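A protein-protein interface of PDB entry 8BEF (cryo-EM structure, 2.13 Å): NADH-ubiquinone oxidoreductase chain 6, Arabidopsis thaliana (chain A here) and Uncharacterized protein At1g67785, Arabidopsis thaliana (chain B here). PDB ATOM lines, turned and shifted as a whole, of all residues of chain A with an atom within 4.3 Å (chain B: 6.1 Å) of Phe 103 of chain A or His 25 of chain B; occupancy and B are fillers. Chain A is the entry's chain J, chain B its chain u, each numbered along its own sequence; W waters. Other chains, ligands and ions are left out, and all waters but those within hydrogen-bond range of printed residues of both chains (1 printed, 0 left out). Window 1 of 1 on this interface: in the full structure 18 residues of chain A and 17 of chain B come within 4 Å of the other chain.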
ATOM      1  N   TRP A  98      12.635  -0.515 -11.020  1.00  0.00           N
ATOM      2  CA  TRP A  98      12.860  -1.957 -11.030  1.00  0.00           C
ATOM      3  C   TRP A  98      13.176  -2.483  -9.634  1.00  0.00           C
ATOM      4  O   TRP A  98      12.550  -3.441  -9.169  1.00  0.00           O
ATOM      5  CB  TRP A  98      13.989  -2.311 -11.989  1.00  0.00           C
ATOM      6  CG  TRP A  98      14.298  -3.768 -12.003  1.00  0.00           C
ATOM      7  CD1 TRP A  98      13.579  -4.759 -12.605  1.00  0.00           C
ATOM      8  CD2 TRP A  98      15.398  -4.410 -11.351  1.00  0.00           C
ATOM      9  NE1 TRP A  98      14.175  -5.974 -12.386  1.00  0.00           N
ATOM     10  CE2 TRP A  98      15.292  -5.788 -11.616  1.00  0.00           C
ATOM     11  CE3 TRP A  98      16.465  -3.952 -10.574  1.00  0.00           C
ATOM     12  CZ2 TRP A  98      16.214  -6.712 -11.132  1.00  0.00           C
ATOM     13  CZ3 TRP A  98      17.378  -4.871 -10.095  1.00  0.00           C
ATOM     14  CH2 TRP A  98      17.247  -6.236 -10.376  1.00  0.00           C
ATOM     15  N   TRP A  99      14.138  -1.860  -8.949  1.00  0.00           N
ATOM     16  CA  TRP A  99      14.574  -2.354  -7.644  1.00  0.00           C
ATOM     17  C   TRP A  99      13.472  -2.256  -6.600  1.00  0.00           C
ATOM     18  O   TRP A  99      13.388  -3.094  -5.696  1.00  0.00           O
ATOM     19  CB  TRP A  99      15.805  -1.579  -7.178  1.00  0.00           C
ATOM     20  CG  TRP A  99      16.165  -1.845  -5.747  1.00  0.00           C
ATOM     21  CD1 TRP A  99      16.197  -0.934  -4.737  1.00  0.00           C
ATOM     22  CD2 TRP A  99      16.519  -3.107  -5.161  1.00  0.00           C
ATOM     23  NE1 TRP A  99      16.560  -1.541  -3.560  1.00  0.00           N
ATOM     24  CE2 TRP A  99      16.763  -2.875  -3.793  1.00  0.00           C
ATOM     25  CE3 TRP A  99      16.661  -4.406  -5.660  1.00  0.00           C
ATOM     26  CZ2 TRP A  99      17.138  -3.892  -2.918  1.00  0.00           C
ATOM     27  CZ3 TRP A  99      17.033  -5.414  -4.789  1.00  0.00           C
ATOM     28  CH2 TRP A  99      17.268  -5.151  -3.434  1.00  0.00           C
ATOM     29  N   GLU A 100      12.619  -1.253  -6.709  1.00  0.00           N
ATOM     30  CA  GLU A 100      11.577  -1.062  -5.716  1.00  0.00           C
ATOM     31  C   GLU A 100      10.325  -1.863  -6.013  1.00  0.00           C
ATOM     32  O   GLU A 100       9.702  -2.403  -5.096  1.00  0.00           O
ATOM     33  CB  GLU A 100      11.186   0.410  -5.665  1.00  0.00           C
ATOM     34  CG  GLU A 100      10.245   0.703  -4.560  1.00  0.00           C
ATOM     35  CD  GLU A 100      10.973   0.835  -3.267  1.00  0.00           C
ATOM     36  OE1 GLU A 100      12.001   1.536  -3.249  1.00  0.00           O
ATOM     37  OE2 GLU A 100      10.537   0.204  -2.283  1.00  0.00           O
ATOM     38  N   MET A 101       9.963  -1.955  -7.266  1.00  0.00           N
ATOM     39  CA  MET A 101       8.583  -2.159  -7.646  1.00  0.00           C
ATOM     40  C   MET A 101       8.325  -3.535  -8.251  1.00  0.00           C
ATOM     41  O   MET A 101       7.183  -3.996  -8.245  1.00  0.00           O
ATOM     42  CB  MET A 101       8.182  -1.015  -8.594  1.00  0.00           C
ATOM     43  CG  MET A 101       7.088  -1.260  -9.509  1.00  0.00           C
ATOM     44  SD  MET A 101       5.639  -0.389  -8.878  1.00  0.00           S
ATOM     45  CE  MET A 101       6.059   1.346  -9.099  1.00  0.00           C
ATOM     46  N   PHE A 102       9.358  -4.207  -8.766  1.00  0.00           N
ATOM     47  CA  PHE A 102       9.260  -5.629  -9.096  1.00  0.00           C
ATOM     48  C   PHE A 102       9.354  -6.521  -7.867  1.00  0.00           C
ATOM     49  O   PHE A 102       8.965  -7.688  -7.938  1.00  0.00           O
ATOM     50  CB  PHE A 102      10.358  -6.038 -10.081  1.00  0.00           C
ATOM     51  CG  PHE A 102      10.155  -5.531 -11.472  1.00  0.00           C
ATOM     52  CD1 PHE A 102      10.289  -4.182 -11.755  1.00  0.00           C
ATOM     53  CD2 PHE A 102       9.854  -6.399 -12.504  1.00  0.00           C
ATOM     54  CE1 PHE A 102      10.106  -3.715 -13.037  1.00  0.00           C
ATOM     55  CE2 PHE A 102       9.674  -5.935 -13.788  1.00  0.00           C
ATOM     56  CZ  PHE A 102       9.801  -4.595 -14.053  1.00  0.00           C
ATOM     57  N   PHE A 103       9.860  -5.997  -6.748  1.00  0.00           N
ATOM     58  CA  PHE A 103      10.114  -6.786  -5.546  1.00  0.00           C
ATOM     59  C   PHE A 103       9.281  -6.325  -4.360  1.00  0.00           C
ATOM     60  O   PHE A 103       9.572  -6.715  -3.225  1.00  0.00           O
ATOM     61  CB  PHE A 103      11.605  -6.737  -5.191  1.00  0.00           C
ATOM     62  CG  PHE A 103      12.510  -7.062  -6.346  1.00  0.00           C
ATOM     63  CD1 PHE A 103      12.618  -8.362  -6.812  1.00  0.00           C
ATOM     64  CD2 PHE A 103      13.234  -6.066  -6.979  1.00  0.00           C
ATOM     65  CE1 PHE A 103      13.443  -8.665  -7.881  1.00  0.00           C
ATOM     66  CE2 PHE A 103      14.058  -6.363  -8.047  1.00  0.00           C
ATOM     67  CZ  PHE A 103      14.161  -7.665  -8.501  1.00  0.00           C
ATOM     68  N   ILE A 104       8.254  -5.506  -4.595  1.00  0.00           N
ATOM     69  CA  ILE A 104       7.455  -4.951  -3.507  1.00  0.00           C
ATOM     70  C   ILE A 104       6.678  -6.043  -2.782  1.00  0.00           C
ATOM     71  O   ILE A 104       6.473  -5.963  -1.566  1.00  0.00           O
ATOM     72  CB  ILE A 104       6.532  -3.847  -4.063  1.00  0.00           C
ATOM     73  CG1 ILE A 104       5.571  -3.320  -3.001  1.00  0.00           C
ATOM     74  CG2 ILE A 104       5.768  -4.347  -5.246  1.00  0.00           C
ATOM     75  CD1 ILE A 104       5.200  -1.875  -3.201  1.00  0.00           C
ATOM     76  N   LEU A 105       6.245  -7.077  -3.503  1.00  0.00           N
ATOM     77  CA  LEU A 105       5.490  -8.168  -2.902  1.00  0.00           C
ATOM     78  C   LEU A 105       6.365  -9.170  -2.158  1.00  0.00           C
ATOM     79  O   LEU A 105       5.826 -10.003  -1.421  1.00  0.00           O
ATOM     80  CB  LEU A 105       4.686  -8.912  -3.975  1.00  0.00           C
ATOM     81  CG  LEU A 105       3.677  -8.149  -4.837  1.00  0.00           C
ATOM     82  CD1 LEU A 105       2.701  -9.115  -5.495  1.00  0.00           C
ATOM     83  CD2 LEU A 105       2.925  -7.116  -4.025  1.00  0.00           C
ATOM     84  N   ASP A 106       7.689  -9.112  -2.327  1.00  0.00           N
ATOM     85  CA  ASP A 106       8.549 -10.180  -1.824  1.00  0.00           C
ATOM     86  C   ASP A 106       8.503 -10.287  -0.304  1.00  0.00           C
ATOM     87  O   ASP A 106       8.493 -11.395   0.241  1.00  0.00           O
ATOM     88  CB  ASP A 106       9.982  -9.969  -2.312  1.00  0.00           C
ATOM     89  CG  ASP A 106      10.116 -10.167  -3.811  1.00  0.00           C
ATOM     90  OD1 ASP A 106       9.164  -9.823  -4.542  1.00  0.00           O
ATOM     91  OD2 ASP A 106      11.164 -10.673  -4.258  1.00  0.00           O
ATOM     92  N   SER B  20      16.200 -15.292 -15.461  1.00  0.00           N
ATOM     93  CA  SER B  20      17.101 -14.654 -14.503  1.00  0.00           C
ATOM     94  C   SER B  20      16.327 -14.018 -13.352  1.00  0.00           C
ATOM     95  O   SER B  20      16.744 -14.095 -12.186  1.00  0.00           O
ATOM     96  CB  SER B  20      17.963 -13.607 -15.208  1.00  0.00           C
ATOM     97  OG  SER B  20      18.349 -14.042 -16.496  1.00  0.00           O
ATOM     98  N   MET B  21      15.205 -13.368 -13.663  1.00  0.00           N
ATOM     99  CA  MET B  21      14.365 -12.791 -12.619  1.00  0.00           C
ATOM    100  C   MET B  21      13.870 -13.869 -11.661  1.00  0.00           C
ATOM    101  O   MET B  21      13.775 -13.643 -10.448  1.00  0.00           O
ATOM    102  CB  MET B  21      13.185 -12.049 -13.248  1.00  0.00           C
ATOM    103  CG  MET B  21      13.429 -10.570 -13.544  1.00  0.00           C
ATOM    104  SD  MET B  21      14.394  -9.676 -12.307  1.00  0.00           S
ATOM    105  CE  MET B  21      16.028  -9.713 -13.044  1.00  0.00           C
ATOM    106  N   ASP B  22      13.538 -15.045 -12.195  1.00  0.00           N
ATOM    107  CA  ASP B  22      13.146 -16.169 -11.348  1.00  0.00           C
ATOM    108  C   ASP B  22      14.257 -16.526 -10.367  1.00  0.00           C
ATOM    109  O   ASP B  22      14.008 -16.752  -9.172  1.00  0.00           O
ATOM    110  CB  ASP B  22      12.799 -17.381 -12.211  1.00  0.00           C
ATOM    111  CG  ASP B  22      11.450 -17.256 -12.883  1.00  0.00           C
ATOM    112  OD1 ASP B  22      10.939 -16.124 -13.001  1.00  0.00           O
ATOM    113  OD2 ASP B  22      10.898 -18.298 -13.299  1.00  0.00           O
ATOM    114  N   LYS B  23      15.493 -16.594 -10.866  1.00  0.00           N
ATOM    115  CA  LYS B  23      16.624 -16.867  -9.978  1.00  0.00           C
ATOM    116  C   LYS B  23      16.741 -15.799  -8.895  1.00  0.00           C
ATOM    117  O   LYS B  23      17.035 -16.107  -7.731  1.00  0.00           O
ATOM    118  CB  LYS B  23      17.921 -16.956 -10.778  1.00  0.00           C
ATOM    119  CG  LYS B  23      18.002 -18.154 -11.698  1.00  0.00           C
ATOM    120  CD  LYS B  23      19.277 -18.129 -12.516  1.00  0.00           C
ATOM    121  CE  LYS B  23      19.557 -19.487 -13.138  1.00  0.00           C
ATOM    122  NZ  LYS B  23      18.818 -20.573 -12.440  1.00  0.00           N
ATOM    123  N   VAL B  24      16.514 -14.535  -9.263  1.00  0.00           N
ATOM    124  CA  VAL B  24      16.564 -13.446  -8.286  1.00  0.00           C
ATOM    125  C   VAL B  24      15.512 -13.646  -7.199  1.00  0.00           C
ATOM    126  O   VAL B  24      15.779 -13.435  -6.006  1.00  0.00           O
ATOM    127  CB  VAL B  24      16.394 -12.085  -8.985  1.00  0.00           C
ATOM    128  CG1 VAL B  24      16.301 -10.971  -7.956  1.00  0.00           C
ATOM    129  CG2 VAL B  24      17.545 -11.827  -9.940  1.00  0.00           C
ATOM    130  N   HIS B  25      14.295 -14.020  -7.593  1.00  0.00           N
ATOM    131  CA  HIS B  25      13.237 -14.228  -6.607  1.00  0.00           C
ATOM    132  C   HIS B  25      13.588 -15.369  -5.660  1.00  0.00           C
ATOM    133  O   HIS B  25      13.337 -15.281  -4.450  1.00  0.00           O
ATOM    134  CB  HIS B  25      11.903 -14.488  -7.303  1.00  0.00           C
ATOM    135  CG  HIS B  25      11.409 -13.326  -8.107  1.00  0.00           C
ATOM    136  ND1 HIS B  25      11.315 -12.053  -7.590  1.00  0.00           N
ATOM    137  CD2 HIS B  25      10.987 -13.244  -9.390  1.00  0.00           C
ATOM    138  CE1 HIS B  25      10.861 -11.234  -8.522  1.00  0.00           C
ATOM    139  NE2 HIS B  25      10.648 -11.934  -9.622  1.00  0.00           N
ATOM    140  N   VAL B  26      14.178 -16.444  -6.192  1.00  0.00           N
ATOM    141  CA  VAL B  26      14.620 -17.542  -5.333  1.00  0.00           C
ATOM    142  C   VAL B  26      15.671 -17.057  -4.340  1.00  0.00           C
ATOM    143  O   VAL B  26      15.622 -17.391  -3.148  1.00  0.00           O
ATOM    144  CB  VAL B  26      15.143 -18.717  -6.180  1.00  0.00           C
ATOM    145  CG1 VAL B  26      15.854 -19.734  -5.298  1.00  0.00           C
ATOM    146  CG2 VAL B  26      13.999 -19.376  -6.918  1.00  0.00           C
ATOM    147  N   TRP B  27      16.637 -16.264  -4.812  1.00  0.00           N
ATOM    148  CA  TRP B  27      17.632 -15.694  -3.906  1.00  0.00           C
ATOM    149  C   TRP B  27      16.981 -14.886  -2.791  1.00  0.00           C
ATOM    150  O   TRP B  27      17.338 -15.029  -1.617  1.00  0.00           O
ATOM    151  CB  TRP B  27      18.620 -14.820  -4.675  1.00  0.00           C
ATOM    152  CG  TRP B  27      19.872 -14.568  -3.909  1.00  0.00           C
ATOM    153  CD1 TRP B  27      20.970 -15.368  -3.841  1.00  0.00           C
ATOM    154  CD2 TRP B  27      20.145 -13.440  -3.070  1.00  0.00           C
ATOM    155  NE1 TRP B  27      21.918 -14.804  -3.026  1.00  0.00           N
ATOM    156  CE2 TRP B  27      21.436 -13.618  -2.540  1.00  0.00           C
ATOM    157  CE3 TRP B  27      19.425 -12.293  -2.724  1.00  0.00           C
ATOM    158  CZ2 TRP B  27      22.022 -12.695  -1.679  1.00  0.00           C
ATOM    159  CZ3 TRP B  27      20.011 -11.375  -1.869  1.00  0.00           C
ATOM    160  CH2 TRP B  27      21.296 -11.582  -1.357  1.00  0.00           C
ATOM    161  N   ILE B  28      16.028 -14.020  -3.143  1.00  0.00           N
ATOM    162  CA  ILE B  28      15.398 -13.173  -2.132  1.00  0.00           C
ATOM    163  C   ILE B  28      14.655 -14.026  -1.112  1.00  0.00           C
ATOM    164  O   ILE B  28      14.719 -13.769   0.098  1.00  0.00           O
ATOM    165  CB  ILE B  28      14.470 -12.137  -2.792  1.00  0.00           C
ATOM    166  CG1 ILE B  28      15.295 -11.063  -3.499  1.00  0.00           C
ATOM    167  CG2 ILE B  28      13.563 -11.493  -1.755  1.00  0.00           C
ATOM    168  CD1 ILE B  28      14.597 -10.440  -4.671  1.00  0.00           C
ATOM    169  N   ALA B  29      13.947 -15.057  -1.577  1.00  0.00           N
ATOM    170  CA  ALA B  29      13.234 -15.937  -0.655  1.00  0.00           C
ATOM    171  C   ALA B  29      14.195 -16.665   0.281  1.00  0.00           C
ATOM    172  O   ALA B  29      13.910 -16.820   1.474  1.00  0.00           O
ATOM    173  CB  ALA B  29      12.385 -16.941  -1.432  1.00  0.00           C
ATOM    174  N   LEU B  30      15.340 -17.116  -0.238  1.00  0.00           N
ATOM    175  CA  LEU B  30      16.272 -17.881   0.587  1.00  0.00           C
ATOM    176  C   LEU B  30      16.899 -17.053   1.702  1.00  0.00           C
ATOM    177  O   LEU B  30      17.420 -17.631   2.660  1.00  0.00           O
ATOM    178  CB  LEU B  30      17.375 -18.492  -0.278  1.00  0.00           C
ATOM    179  CG  LEU B  30      16.984 -19.746  -1.060  1.00  0.00           C
ATOM    180  CD1 LEU B  30      17.892 -19.938  -2.259  1.00  0.00           C
ATOM    181  CD2 LEU B  30      17.013 -20.968  -0.163  1.00  0.00           C
HETATM  182  O   HOH W   1      11.365 -13.554  -2.899  1.00  0.00           O
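The indole nitrogen (NE1) of Trp 98 of chain A sits close to the side-chain sulfur (SD) of Met 21 of chain B, at 3.7 Å.
Among the printed residues, pairs that only touch across the chains: Phe 103 of chain A with Val 24 of chain B (3.7 Å), Phe 103 of chain A with His 25 of chain B (3.7 Å), Phe 103 of chain A with Ile 28 of chain B (3.6 Å), Asp 106 of chain A with His 25 of chain B (3.6 Å) and Asp 106 of chain A with Ile 28 of chain B (3.5 Å).
Glu 100 of chain A touches none of the printed residues of chain B.
Of the printed residues of chain B, Asp 106 of chain A touches His 25 (3.6 Å) and Ile 28 (3.5 Å).
Ser 20 of chain B touches none of the printed residues of chain A.
Printed residues of chain A within 4 Å of Ile 28 of chain B: Phe 103 (3.6 Å) and Asp 106 (3.5 Å).
The nearest residue of chain B that does not touch Phe 103 of chain A is Met 21 of chain B (4.3 Å).
The nearest printed residue of chain B that does not touch Asp 106 of chain A is Val 24 of chain B (5.7 Å).
Hydrophobic or aromatic side chains of chain A within 4 Å of the printed part of chain B: Trp 98 and Phe 103.
Of the 11 printed residues of chain B, 4 touch a printed residue of chain A.
Hydrophobic or aromatic side chains of chain B within 4 Å of the printed part of chain A: Met 21, Val 24, His 25 and Ile 28.
Among the printed residues, 6 pairs touch across the chains.
Among the printed residues, no Asp or Glu carboxylate lies within 4 Å of a Lys or Arg side-chain nitrogen of the other chain.
Water W1 lies within hydrogen-bond range of the backbone carbonyl oxygen of His 25 of chain B, the side-chain carboxylate of Asp 106 of chain A and the backbone NH of Ala 29 of chain B.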
